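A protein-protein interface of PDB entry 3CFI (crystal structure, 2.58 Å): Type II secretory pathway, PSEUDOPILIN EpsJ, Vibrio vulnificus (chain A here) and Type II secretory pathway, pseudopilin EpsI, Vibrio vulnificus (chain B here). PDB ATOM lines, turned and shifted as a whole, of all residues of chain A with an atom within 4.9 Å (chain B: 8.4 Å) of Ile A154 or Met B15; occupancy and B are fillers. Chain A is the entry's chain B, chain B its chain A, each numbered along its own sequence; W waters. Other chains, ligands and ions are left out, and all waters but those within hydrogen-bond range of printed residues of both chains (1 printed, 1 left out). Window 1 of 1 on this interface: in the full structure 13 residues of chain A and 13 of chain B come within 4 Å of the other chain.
Hydrophobic or aromatic side chains of chain B within 4 Å of the printed part of chain A: Met B11, Phe B12, Met B15 and Leu B40. Printed residues of chain A that touch a printed residue of chain B: Leu A14, Leu A18, Tyr A151, Lys A153, Ile A154, Ala A155 and Arg A156. Among the printed residues, 17 pairs touch across the chains. Among the printed residues, Asp or Glu carboxylates within 4 Å of a Lys or Arg side-chain nitrogen of the other chain: Arg A156 with Asp B18 (3.5 Å).
Water W1 lies within hydrogen-bond range of N of Gly B42 (2.7 Å), O of Lys A153 (2.9 Å) and N of Ala B41 (3.4 Å).
Printed residues of chain B within 4 Å of Ile A154: Phe B12 (3.9 Å), Met B15 (3.2 Å), Leu B40 (3.999 Å) and Ala B41 (3.7 Å). Of the printed residues of chain B, Ala A155 touches Asn B19 and Leu B40. Printed residues of chain A within 4 Å of Met B11: Leu A14 (3.4 Å). Printed residues of chain A within 4 Å of Phe B12: Leu A14 (3.9 Å) and Ile A154 (3.9 Å). Ala B13 touches none of the printed residues of chain A. Printed residues of chain A within 4 Å of Met B15: Leu A18 (3.3 Å), Ile A154 (3.2 Å) and Arg A156 (3.99 Å). Gln B20 touches none of the printed residues of chain A. Printed residues of chain A within 4 Å of Ala B41: Tyr A151, Lys A153 and Ile A154. Printed residues of chain A within 4 Å of Gly B42: Tyr A151. The nearest printed residue of chain A that does not touch Asp B18 is Ala A155 (7.6 Å).
CD2 of Leu A14 touches CE of Met B11, 3.4 Å away. CD1 of Leu A18 touches CE of Met B15 (3.3 Å). Tyr A151 touches Glu B8. O of Lys A153 touches CA of Leu B40, at 3.7 Å. Ile A154 touches Phe B12. Ile A154 touches Met B15 (CG2 to CE, 3.2 Å). CG1 of Ile A154 touches CD2 of Leu B40, at 3.999 Å. Ile A154 touches Ala B41. Arg A156 touches Met B15. Arg A156 touches Asn B19.
O of Met B15 lies close to OD1 of Asn B19 (3.3 Å). ND2 of Asn B19 lies within hydrogen-bond range of OE2 of Glu B38. The backbone carbonyl oxygen (O) of Leu B40 sits at hydrogen-bond distance from the indole nitrogen (NE1) of Trp B45, at 3.1 Å. N of Val A144 lies within hydrogen-bond range of O of Arg A156 (2.9 Å). OE1 of Glu A145 lies within salt-bridge range of NZ of Lys A153 (3.0 Å). N of Leu A146 sits at hydrogen-bond distance from O of Ile A154, at 2.8 Å.
The side-chain carboxylate (OD2) of Asp B18 lies within salt-bridge range of the guanidinium group (NH2) of Arg A156. ND2 of Asn B19 is in hydrogen-bond range of O of Ala A155, at 3.0 Å. The backbone carbonyl oxygen (O) of Lys A153 lies within hydrogen-bond range of the backbone NH (N) of Ala B41 (2.9 Å). N of Gly B42 lies within hydrogen-bond range of O of Tyr A151, 3.2 Å away. The backbone carbonyl oxygen of Tyr A151 sits close to the backbone carbonyl oxygen of Ala B41.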
ATOM      1  N   LEU A  14       5.793  -7.283   1.430  1.00  0.00           N
ATOM      2  CA  LEU A  14       4.773  -6.554   0.677  1.00  0.00           C
ATOM      3  C   LEU A  14       4.284  -5.323   1.452  1.00  0.00           C
ATOM      4  O   LEU A  14       4.095  -4.249   0.872  1.00  0.00           O
ATOM      5  CB  LEU A  14       3.598  -7.484   0.330  1.00  0.00           C
ATOM      6  CG  LEU A  14       2.448  -6.937  -0.530  1.00  0.00           C
ATOM      7  CD1 LEU A  14       2.937  -6.408  -1.871  1.00  0.00           C
ATOM      8  CD2 LEU A  14       1.382  -8.003  -0.746  1.00  0.00           C
ATOM      9  N   LEU A  18       4.311  -1.463   0.410  1.00  0.00           N
ATOM     10  CA  LEU A  18       3.056  -0.712   0.347  1.00  0.00           C
ATOM     11  C   LEU A  18       3.088   0.535   1.227  1.00  0.00           C
ATOM     12  O   LEU A  18       2.653   1.596   0.800  1.00  0.00           O
ATOM     13  CB  LEU A  18       1.859  -1.600   0.716  1.00  0.00           C
ATOM     14  CG  LEU A  18       1.510  -2.742  -0.255  1.00  0.00           C
ATOM     15  CD1 LEU A  18       0.382  -3.614   0.304  1.00  0.00           C
ATOM     16  CD2 LEU A  18       1.136  -2.217  -1.630  1.00  0.00           C
ATOM     17  N   VAL A 144      -2.059   2.506  -8.117  1.00  0.00           N
ATOM     18  CA  VAL A 144      -0.788   1.841  -8.417  1.00  0.00           C
ATOM     19  C   VAL A 144      -0.976   0.326  -8.391  1.00  0.00           C
ATOM     20  O   VAL A 144      -1.317  -0.234  -7.351  1.00  0.00           O
ATOM     21  CB  VAL A 144       0.300   2.235  -7.409  1.00  0.00           C
ATOM     22  CG1 VAL A 144       1.623   1.587  -7.770  1.00  0.00           C
ATOM     23  CG2 VAL A 144       0.443   3.752  -7.357  1.00  0.00           C
ATOM     24  N   GLU A 145      -0.759  -0.318  -9.538  1.00  0.00           N
ATOM     25  CA  GLU A 145      -0.918  -1.766  -9.682  1.00  0.00           C
ATOM     26  C   GLU A 145       0.432  -2.465  -9.858  1.00  0.00           C
ATOM     27  O   GLU A 145       1.166  -2.188 -10.809  1.00  0.00           O
ATOM     28  CB  GLU A 145      -1.821  -2.104 -10.874  1.00  0.00           C
ATOM     29  CG  GLU A 145      -2.285  -3.567 -10.887  1.00  0.00           C
ATOM     30  CD  GLU A 145      -2.881  -4.012 -12.213  1.00  0.00           C
ATOM     31  OE1 GLU A 145      -2.153  -4.002 -13.231  1.00  0.00           O
ATOM     32  OE2 GLU A 145      -4.074  -4.397 -12.227  1.00  0.00           O
ATOM     33  N   LEU A 146       0.736  -3.387  -8.947  1.00  0.00           N
ATOM     34  CA  LEU A 146       1.963  -4.184  -8.997  1.00  0.00           C
ATOM     35  C   LEU A 146       1.636  -5.621  -9.397  1.00  0.00           C
ATOM     36  O   LEU A 146       0.761  -6.244  -8.798  1.00  0.00           O
ATOM     37  CB  LEU A 146       2.645  -4.186  -7.626  1.00  0.00           C
ATOM     38  CG  LEU A 146       3.092  -2.822  -7.088  1.00  0.00           C
ATOM     39  CD1 LEU A 146       3.453  -2.907  -5.623  1.00  0.00           C
ATOM     40  CD2 LEU A 146       4.262  -2.290  -7.900  1.00  0.00           C
ATOM     41  N   LEU A 148       2.965  -9.103  -9.163  1.00  0.00           N
ATOM     42  CA  LEU A 148       3.928  -9.983  -8.490  1.00  0.00           C
ATOM     43  C   LEU A 148       3.960 -11.366  -9.142  1.00  0.00           C
ATOM     44  O   LEU A 148       2.940 -11.860  -9.618  1.00  0.00           O
ATOM     45  CB  LEU A 148       3.571 -10.142  -7.007  1.00  0.00           C
ATOM     46  CG  LEU A 148       3.352  -8.880  -6.165  1.00  0.00           C
ATOM     47  CD1 LEU A 148       3.314  -9.237  -4.679  1.00  0.00           C
ATOM     48  CD2 LEU A 148       4.423  -7.851  -6.435  1.00  0.00           C
ATOM     49  N   TYR A 151       1.857 -13.730  -6.361  1.00  0.00           N
ATOM     50  CA  TYR A 151       0.480 -13.329  -6.058  1.00  0.00           C
ATOM     51  C   TYR A 151      -0.264 -12.708  -7.240  1.00  0.00           C
ATOM     52  O   TYR A 151      -1.483 -12.603  -7.205  1.00  0.00           O
ATOM     53  CB  TYR A 151       0.479 -12.340  -4.892  1.00  0.00           C
ATOM     54  CG  TYR A 151       0.812 -12.953  -3.547  1.00  0.00           C
ATOM     55  CD1 TYR A 151       0.139 -14.084  -3.086  1.00  0.00           C
ATOM     56  CD2 TYR A 151       1.768 -12.377  -2.716  1.00  0.00           C
ATOM     57  CE1 TYR A 151       0.426 -14.640  -1.846  1.00  0.00           C
ATOM     58  CE2 TYR A 151       2.065 -12.928  -1.474  1.00  0.00           C
ATOM     59  CZ  TYR A 151       1.392 -14.061  -1.047  1.00  0.00           C
ATOM     60  OH  TYR A 151       1.678 -14.614   0.180  1.00  0.00           O
ATOM     61  N   GLY A 152       0.453 -12.295  -8.282  1.00  0.00           N
ATOM     62  CA  GLY A 152      -0.185 -11.674  -9.443  1.00  0.00           C
ATOM     63  C   GLY A 152      -0.471 -10.207  -9.193  1.00  0.00           C
ATOM     64  O   GLY A 152       0.302  -9.535  -8.518  1.00  0.00           O
ATOM     65  N   LYS A 153      -1.580  -9.711  -9.729  1.00  0.00           N
ATOM     66  CA  LYS A 153      -1.909  -8.290  -9.665  1.00  0.00           C
ATOM     67  C   LYS A 153      -2.439  -7.878  -8.299  1.00  0.00           C
ATOM     68  O   LYS A 153      -3.426  -8.433  -7.814  1.00  0.00           O
ATOM     69  CB  LYS A 153      -2.952  -7.919 -10.725  1.00  0.00           C
ATOM     70  CG  LYS A 153      -2.401  -7.822 -12.144  1.00  0.00           C
ATOM     71  CD  LYS A 153      -3.522  -7.848 -13.175  1.00  0.00           C
ATOM     72  CE  LYS A 153      -2.981  -7.791 -14.591  1.00  0.00           C
ATOM     73  NZ  LYS A 153      -2.427  -6.457 -14.925  1.00  0.00           N
ATOM     74  N   ILE A 154      -1.779  -6.898  -7.690  1.00  0.00           N
ATOM     75  CA  ILE A 154      -2.289  -6.226  -6.505  1.00  0.00           C
ATOM     76  C   ILE A 154      -2.309  -4.729  -6.756  1.00  0.00           C
ATOM     77  O   ILE A 154      -1.320  -4.169  -7.222  1.00  0.00           O
ATOM     78  CB  ILE A 154      -1.377  -6.515  -5.295  1.00  0.00           C
ATOM     79  CG1 ILE A 154      -1.649  -7.919  -4.759  1.00  0.00           C
ATOM     80  CG2 ILE A 154      -1.570  -5.473  -4.196  1.00  0.00           C
ATOM     81  CD1 ILE A 154      -0.556  -8.430  -3.865  1.00  0.00           C
ATOM     82  N   ALA A 155      -3.431  -4.083  -6.440  1.00  0.00           N
ATOM     83  CA  ALA A 155      -3.589  -2.649  -6.686  1.00  0.00           C
ATOM     84  C   ALA A 155      -3.878  -1.887  -5.403  1.00  0.00           C
ATOM     85  O   ALA A 155      -4.490  -2.418  -4.478  1.00  0.00           O
ATOM     86  CB  ALA A 155      -4.699  -2.408  -7.691  1.00  0.00           C
ATOM     87  N   ARG A 156      -3.430  -0.632  -5.366  1.00  0.00           N
ATOM     88  CA  ARG A 156      -3.667   0.253  -4.234  1.00  0.00           C
ATOM     89  C   ARG A 156      -4.063   1.651  -4.715  1.00  0.00           C
ATOM     90  O   ARG A 156      -3.347   2.267  -5.506  1.00  0.00           O
ATOM     91  CB  ARG A 156      -2.412   0.324  -3.368  1.00  0.00           C
ATOM     92  CG  ARG A 156      -2.615   1.101  -2.081  1.00  0.00           C
ATOM     93  CD  ARG A 156      -1.616   0.729  -0.996  1.00  0.00           C
ATOM     94  NE  ARG A 156      -2.044   1.260   0.295  1.00  0.00           N
ATOM     95  CZ  ARG A 156      -2.759   0.591   1.199  1.00  0.00           C
ATOM     96  NH1 ARG A 156      -3.152  -0.660   0.987  1.00  0.00           N
ATOM     97  NH2 ARG A 156      -3.088   1.188   2.341  1.00  0.00           N
ATOM     98  N   GLU B   8      -2.828 -14.073   4.939  1.00  0.00           N
ATOM     99  CA  GLU B   8      -2.941 -13.571   3.569  1.00  0.00           C
ATOM    100  C   GLU B   8      -4.326 -12.961   3.370  1.00  0.00           C
ATOM    101  O   GLU B   8      -4.454 -11.823   2.915  1.00  0.00           O
ATOM    102  CB  GLU B   8      -2.763 -14.692   2.544  1.00  0.00           C
ATOM    103  CG  GLU B   8      -1.347 -15.198   2.366  1.00  0.00           C
ATOM    104  CD  GLU B   8      -1.250 -16.222   1.246  1.00  0.00           C
ATOM    105  OE1 GLU B   8      -1.928 -16.025   0.213  1.00  0.00           O
ATOM    106  OE2 GLU B   8      -0.502 -17.218   1.390  1.00  0.00           O
ATOM    107  N   GLN B   9      -5.352 -13.739   3.718  1.00  0.00           N
ATOM    108  CA  GLN B   9      -6.751 -13.328   3.570  1.00  0.00           C
ATOM    109  C   GLN B   9      -7.057 -12.036   4.334  1.00  0.00           C
ATOM    110  O   GLN B   9      -7.758 -11.161   3.828  1.00  0.00           O
ATOM    111  CB  GLN B   9      -7.691 -14.451   4.044  1.00  0.00           C
ATOM    112  CG  GLN B   9      -8.981 -14.551   3.235  1.00  0.00           C
ATOM    113  CD  GLN B   9      -9.966 -15.574   3.777  1.00  0.00           C
ATOM    114  OE1 GLN B   9     -10.101 -15.754   4.988  1.00  0.00           O
ATOM    115  NE2 GLN B   9     -10.673 -16.238   2.874  1.00  0.00           N
ATOM    116  N   LYS B  10      -6.519 -11.924   5.546  1.00  0.00           N
ATOM    117  CA  LYS B  10      -6.716 -10.741   6.390  1.00  0.00           C
ATOM    118  C   LYS B  10      -6.116  -9.486   5.756  1.00  0.00           C
ATOM    119  O   LYS B  10      -6.732  -8.421   5.771  1.00  0.00           O
ATOM    120  CB  LYS B  10      -6.105 -10.963   7.778  1.00  0.00           C
ATOM    121  CG  LYS B  10      -6.169  -9.749   8.698  1.00  0.00           C
ATOM    122  CD  LYS B  10      -5.775 -10.102  10.124  1.00  0.00           C
ATOM    123  CE  LYS B  10      -5.448  -8.854  10.933  1.00  0.00           C
ATOM    124  NZ  LYS B  10      -6.529  -7.831  10.853  1.00  0.00           N
ATOM    125  N   MET B  11      -4.915  -9.620   5.204  1.00  0.00           N
ATOM    126  CA  MET B  11      -4.208  -8.499   4.591  1.00  0.00           C
ATOM    127  C   MET B  11      -4.869  -8.059   3.285  1.00  0.00           C
ATOM    128  O   MET B  11      -5.110  -6.867   3.077  1.00  0.00           O
ATOM    129  CB  MET B  11      -2.750  -8.888   4.319  1.00  0.00           C
ATOM    130  CG  MET B  11      -1.868  -7.724   3.900  1.00  0.00           C
ATOM    131  SD  MET B  11      -0.158  -8.182   3.579  1.00  0.00           S
ATOM    132  CE  MET B  11      -0.311  -8.968   1.980  1.00  0.00           C
ATOM    133  N   PHE B  12      -5.155  -9.029   2.415  1.00  0.00           N
ATOM    134  CA  PHE B  12      -5.729  -8.751   1.097  1.00  0.00           C
ATOM    135  C   PHE B  12      -7.161  -8.219   1.181  1.00  0.00           C
ATOM    136  O   PHE B  12      -7.550  -7.362   0.387  1.00  0.00           O
ATOM    137  CB  PHE B  12      -5.672  -9.995   0.199  1.00  0.00           C
ATOM    138  CG  PHE B  12      -4.265 -10.488  -0.085  1.00  0.00           C
ATOM    139  CD1 PHE B  12      -3.238  -9.603  -0.388  1.00  0.00           C
ATOM    140  CD2 PHE B  12      -3.977 -11.845  -0.069  1.00  0.00           C
ATOM    141  CE1 PHE B  12      -1.955 -10.060  -0.652  1.00  0.00           C
ATOM    142  CE2 PHE B  12      -2.691 -12.306  -0.335  1.00  0.00           C
ATOM    143  CZ  PHE B  12      -1.682 -11.409  -0.622  1.00  0.00           C
ATOM    144  N   ALA B  13      -7.940  -8.715   2.137  1.00  0.00           N
ATOM    145  CA  ALA B  13      -9.289  -8.195   2.361  1.00  0.00           C
ATOM    146  C   ALA B  13      -9.237  -6.737   2.822  1.00  0.00           C
ATOM    147  O   ALA B  13     -10.053  -5.922   2.395  1.00  0.00           O
ATOM    148  CB  ALA B  13     -10.033  -9.048   3.377  1.00  0.00           C
ATOM    149  N   ALA B  14      -8.269  -6.417   3.682  1.00  0.00           N
ATOM    150  CA  ALA B  14      -8.068  -5.046   4.157  1.00  0.00           C
ATOM    151  C   ALA B  14      -7.679  -4.114   3.008  1.00  0.00           C
ATOM    152  O   ALA B  14      -8.121  -2.970   2.954  1.00  0.00           O
ATOM    153  CB  ALA B  14      -7.007  -5.008   5.239  1.00  0.00           C
ATOM    154  N   MET B  15      -6.853  -4.611   2.089  1.00  0.00           N
ATOM    155  CA  MET B  15      -6.434  -3.821   0.928  1.00  0.00           C
ATOM    156  C   MET B  15      -7.618  -3.482   0.031  1.00  0.00           C
ATOM    157  O   MET B  15      -7.736  -2.355  -0.438  1.00  0.00           O
ATOM    158  CB  MET B  15      -5.355  -4.549   0.123  1.00  0.00           C
ATOM    159  CG  MET B  15      -4.005  -4.552   0.791  1.00  0.00           C
ATOM    160  SD  MET B  15      -2.763  -5.376  -0.208  1.00  0.00           S
ATOM    161  CE  MET B  15      -2.406  -4.084  -1.397  1.00  0.00           C
ATOM    162  N   VAL B  16      -8.487  -4.461  -0.204  1.00  0.00           N
ATOM    163  CA  VAL B  16      -9.695  -4.242  -1.006  1.00  0.00           C
ATOM    164  C   VAL B  16     -10.632  -3.247  -0.312  1.00  0.00           C
ATOM    165  O   VAL B  16     -11.197  -2.370  -0.957  1.00  0.00           O
ATOM    166  CB  VAL B  16     -10.448  -5.568  -1.311  1.00  0.00           C
ATOM    167  CG1 VAL B  16     -11.750  -5.292  -2.046  1.00  0.00           C
ATOM    168  CG2 VAL B  16      -9.572  -6.506  -2.133  1.00  0.00           C
ATOM    169  N   ALA B  17     -10.774  -3.380   1.005  1.00  0.00           N
ATOM    170  CA  ALA B  17     -11.589  -2.457   1.799  1.00  0.00           C
ATOM    171  C   ALA B  17     -11.084  -1.018   1.693  1.00  0.00           C
ATOM    172  O   ALA B  17     -11.884  -0.089   1.583  1.00  0.00           O
ATOM    173  CB  ALA B  17     -11.618  -2.895   3.259  1.00  0.00           C
ATOM    174  N   ASP B  18      -9.763  -0.840   1.729  1.00  0.00           N
ATOM    175  CA  ASP B  18      -9.153   0.491   1.615  1.00  0.00           C
ATOM    176  C   ASP B  18      -9.413   1.105   0.245  1.00  0.00           C
ATOM    177  O   ASP B  18      -9.702   2.297   0.133  1.00  0.00           O
ATOM    178  CB  ASP B  18      -7.645   0.436   1.860  1.00  0.00           C
ATOM    179  CG  ASP B  18      -7.285   0.131   3.302  1.00  0.00           C
ATOM    180  OD1 ASP B  18      -8.185   0.037   4.163  1.00  0.00           O
ATOM    181  OD2 ASP B  18      -6.078  -0.019   3.575  1.00  0.00           O
ATOM    182  N   ASN B  19      -9.296   0.281  -0.793  1.00  0.00           N
ATOM    183  CA  ASN B  19      -9.517   0.728  -2.165  1.00  0.00           C
ATOM    184  C   ASN B  19     -10.940   1.228  -2.388  1.00  0.00           C
ATOM    185  O   ASN B  19     -11.142   2.270  -3.004  1.00  0.00           O
ATOM    186  CB  ASN B  19      -9.194  -0.400  -3.155  1.00  0.00           C
ATOM    187  CG  ASN B  19      -7.698  -0.631  -3.309  1.00  0.00           C
ATOM    188  OD1 ASN B  19      -6.890  -0.026  -2.606  1.00  0.00           O
ATOM    189  ND2 ASN B  19      -7.323  -1.510  -4.237  1.00  0.00           N
ATOM    190  N   GLN B  20     -11.915   0.485  -1.868  1.00  0.00           N
ATOM    191  CA  GLN B  20     -13.325   0.839  -2.018  1.00  0.00           C
ATOM    192  C   GLN B  20     -13.717   2.028  -1.144  1.00  0.00           C
ATOM    193  O   GLN B  20     -14.545   2.842  -1.543  1.00  0.00           O
ATOM    194  CB  GLN B  20     -14.212  -0.365  -1.701  1.00  0.00           C
ATOM    195  CG  GLN B  20     -13.981  -1.566  -2.622  1.00  0.00           C
ATOM    196  CD  GLN B  20     -14.216  -1.248  -4.087  1.00  0.00           C
ATOM    197  OE1 GLN B  20     -15.105  -0.472  -4.434  1.00  0.00           O
ATOM    198  NE2 GLN B  20     -13.417  -1.852  -4.955  1.00  0.00           N
ATOM    199  N   MET B  21     -13.130   2.120   0.048  1.00  0.00           N
ATOM    200  CA  MET B  21     -13.314   3.290   0.909  1.00  0.00           C
ATOM    201  C   MET B  21     -12.869   4.557   0.191  1.00  0.00           C
ATOM    202  O   MET B  21     -13.516   5.597   0.301  1.00  0.00           O
ATOM    203  CB  MET B  21     -12.540   3.145   2.222  1.00  0.00           C
ATOM    204  CG  MET B  21     -13.255   2.288   3.255  1.00  0.00           C
ATOM    205  SD  MET B  21     -12.427   2.226   4.862  1.00  0.00           S
ATOM    206  CE  MET B  21     -10.928   1.333   4.462  1.00  0.00           C
ATOM    207  N   ALA B  22     -11.766   4.459  -0.544  1.00  0.00           N
ATOM    208  CA  ALA B  22     -11.252   5.580  -1.322  1.00  0.00           C
ATOM    209  C   ALA B  22     -12.183   5.934  -2.479  1.00  0.00           C
ATOM    210  O   ALA B  22     -12.353   7.113  -2.793  1.00  0.00           O
ATOM    211  CB  ALA B  22      -9.854   5.262  -1.843  1.00  0.00           C
ATOM    212  N   GLU B  38     -13.813  -7.165  -6.686  1.00  0.00           N
ATOM    213  CA  GLU B  38     -12.467  -6.671  -6.979  1.00  0.00           C
ATOM    214  C   GLU B  38     -11.477  -7.825  -7.050  1.00  0.00           C
ATOM    215  O   GLU B  38     -11.378  -8.634  -6.131  1.00  0.00           O
ATOM    216  CB  GLU B  38     -12.014  -5.670  -5.913  1.00  0.00           C
ATOM    217  CG  GLU B  38     -10.759  -4.890  -6.291  1.00  0.00           C
ATOM    218  CD  GLU B  38     -10.286  -3.952  -5.196  1.00  0.00           C
ATOM    219  OE1 GLU B  38     -11.123  -3.454  -4.412  1.00  0.00           O
ATOM    220  OE2 GLU B  38      -9.065  -3.706  -5.123  1.00  0.00           O
ATOM    221  N   GLU B  39     -10.745  -7.890  -8.156  1.00  0.00           N
ATOM    222  CA  GLU B  39      -9.722  -8.906  -8.359  1.00  0.00           C
ATOM    223  C   GLU B  39      -8.414  -8.419  -7.730  1.00  0.00           C
ATOM    224  O   GLU B  39      -7.891  -7.373  -8.114  1.00  0.00           O
ATOM    225  CB  GLU B  39      -9.560  -9.172  -9.861  1.00  0.00           C
ATOM    226  CG  GLU B  39      -8.934 -10.515 -10.218  1.00  0.00           C
ATOM    227  CD  GLU B  39      -9.799 -11.709  -9.837  1.00  0.00           C
ATOM    228  OE1 GLU B  39     -11.043 -11.635  -9.973  1.00  0.00           O
ATOM    229  OE2 GLU B  39      -9.224 -12.733  -9.409  1.00  0.00           O
ATOM    230  N   LEU B  40      -7.904  -9.165  -6.753  1.00  0.00           N
ATOM    231  CA  LEU B  40      -6.676  -8.781  -6.041  1.00  0.00           C
ATOM    232  C   LEU B  40      -5.945 -10.010  -5.500  1.00  0.00           C
ATOM    233  O   LEU B  40      -6.574 -10.929  -4.981  1.00  0.00           O
ATOM    234  CB  LEU B  40      -6.994  -7.814  -4.891  1.00  0.00           C
ATOM    235  CG  LEU B  40      -5.804  -7.139  -4.186  1.00  0.00           C
ATOM    236  CD1 LEU B  40      -6.171  -5.743  -3.671  1.00  0.00           C
ATOM    237  CD2 LEU B  40      -5.263  -7.996  -3.048  1.00  0.00           C
ATOM    238  N   ALA B  41      -4.619 -10.012  -5.631  1.00  0.00           N
ATOM    239  CA  ALA B  41      -3.775 -11.130  -5.200  1.00  0.00           C
ATOM    240  C   ALA B  41      -4.206 -12.465  -5.823  1.00  0.00           C
ATOM    241  O   ALA B  41      -4.142 -13.510  -5.179  1.00  0.00           O
ATOM    242  CB  ALA B  41      -3.762 -11.225  -3.679  1.00  0.00           C
ATOM    243  N   GLY B  42      -4.633 -12.419  -7.083  1.00  0.00           N
ATOM    244  CA  GLY B  42      -5.075 -13.614  -7.802  1.00  0.00           C
ATOM    245  C   GLY B  42      -6.318 -14.272  -7.218  1.00  0.00           C
ATOM    246  O   GLY B  42      -6.463 -15.498  -7.271  1.00  0.00           O
ATOM    247  N   GLN B  43      -7.214 -13.457  -6.664  1.00  0.00           N
ATOM    248  CA  GLN B  43      -8.435 -13.948  -6.013  1.00  0.00           C
ATOM    249  C   GLN B  43      -9.559 -12.928  -6.134  1.00  0.00           C
ATOM    250  O   GLN B  43      -9.313 -11.716  -6.180  1.00  0.00           O
ATOM    251  CB  GLN B  43      -8.212 -14.206  -4.521  1.00  0.00           C
ATOM    252  CG  GLN B  43      -7.167 -15.243  -4.174  1.00  0.00           C
ATOM    253  CD  GLN B  43      -6.936 -15.328  -2.678  1.00  0.00           C
ATOM    254  OE1 GLN B  43      -7.853 -15.644  -1.915  1.00  0.00           O
ATOM    255  NE2 GLN B  43      -5.710 -15.034  -2.248  1.00  0.00           N
ATOM    256  N   TRP B  45     -12.702 -10.868  -4.666  1.00  0.00           N
ATOM    257  CA  TRP B  45     -13.161 -10.326  -3.391  1.00  0.00           C
ATOM    258  C   TRP B  45     -14.492  -9.607  -3.574  1.00  0.00           C
ATOM    259  O   TRP B  45     -14.620  -8.742  -4.436  1.00  0.00           O
ATOM    260  CB  TRP B  45     -12.119  -9.361  -2.822  1.00  0.00           C
ATOM    261  CG  TRP B  45     -10.809 -10.021  -2.553  1.00  0.00           C
ATOM    262  CD1 TRP B  45      -9.726 -10.066  -3.385  1.00  0.00           C
ATOM    263  CD2 TRP B  45     -10.442 -10.749  -1.376  1.00  0.00           C
ATOM    264  NE1 TRP B  45      -8.707 -10.774  -2.796  1.00  0.00           N
ATOM    265  CE2 TRP B  45      -9.117 -11.201  -1.562  1.00  0.00           C
ATOM    266  CE3 TRP B  45     -11.101 -11.060  -0.181  1.00  0.00           C
ATOM    267  CZ2 TRP B  45      -8.438 -11.948  -0.598  1.00  0.00           C
ATOM    268  CZ3 TRP B  45     -10.424 -11.803   0.779  1.00  0.00           C
ATOM    269  CH2 TRP B  45      -9.108 -12.240   0.561  1.00  0.00           C
ATOM    270  N   VAL B  64     -17.798  -0.219   4.820  1.00  0.00           N
ATOM    271  CA  VAL B  64     -17.226  -1.031   3.755  1.00  0.00           C
ATOM    272  C   VAL B  64     -16.888  -2.413   4.311  1.00  0.00           C
ATOM    273  O   VAL B  64     -16.082  -2.534   5.237  1.00  0.00           O
ATOM    274  CB  VAL B  64     -15.944  -0.404   3.185  1.00  0.00           C
ATOM    275  CG1 VAL B  64     -15.227  -1.397   2.285  1.00  0.00           C
ATOM    276  CG2 VAL B  64     -16.271   0.870   2.428  1.00  0.00           C
ATOM    277  N   VAL B  66     -15.840  -6.567   3.188  1.00  0.00           N
ATOM    278  CA  VAL B  66     -15.345  -7.448   2.122  1.00  0.00           C
ATOM    279  C   VAL B  66     -15.386  -8.920   2.540  1.00  0.00           C
ATOM    280  O   VAL B  66     -15.073  -9.264   3.680  1.00  0.00           O
ATOM    281  CB  VAL B  66     -13.911  -7.090   1.670  1.00  0.00           C
ATOM    282  CG1 VAL B  66     -13.797  -5.604   1.351  1.00  0.00           C
ATOM    283  CG2 VAL B  66     -12.908  -7.483   2.714  1.00  0.00           C
ATOM    284  N   ILE B  76     -13.750  -8.730   6.964  1.00  0.00           N
ATOM    285  CA  ILE B  76     -13.462  -7.408   7.537  1.00  0.00           C
ATOM    286  C   ILE B  76     -14.604  -6.430   7.258  1.00  0.00           C
ATOM    287  O   ILE B  76     -15.202  -6.460   6.182  1.00  0.00           O
ATOM    288  CB  ILE B  76     -12.148  -6.806   6.974  1.00  0.00           C
ATOM    289  CG1 ILE B  76     -11.780  -5.509   7.707  1.00  0.00           C
ATOM    290  CG2 ILE B  76     -12.276  -6.527   5.491  1.00  0.00           C
ATOM    291  CD1 ILE B  76     -10.386  -5.011   7.394  1.00  0.00           C
HETATM  292  O   HOH W   1      -5.196 -10.499  -8.915  1.00  0.00           O
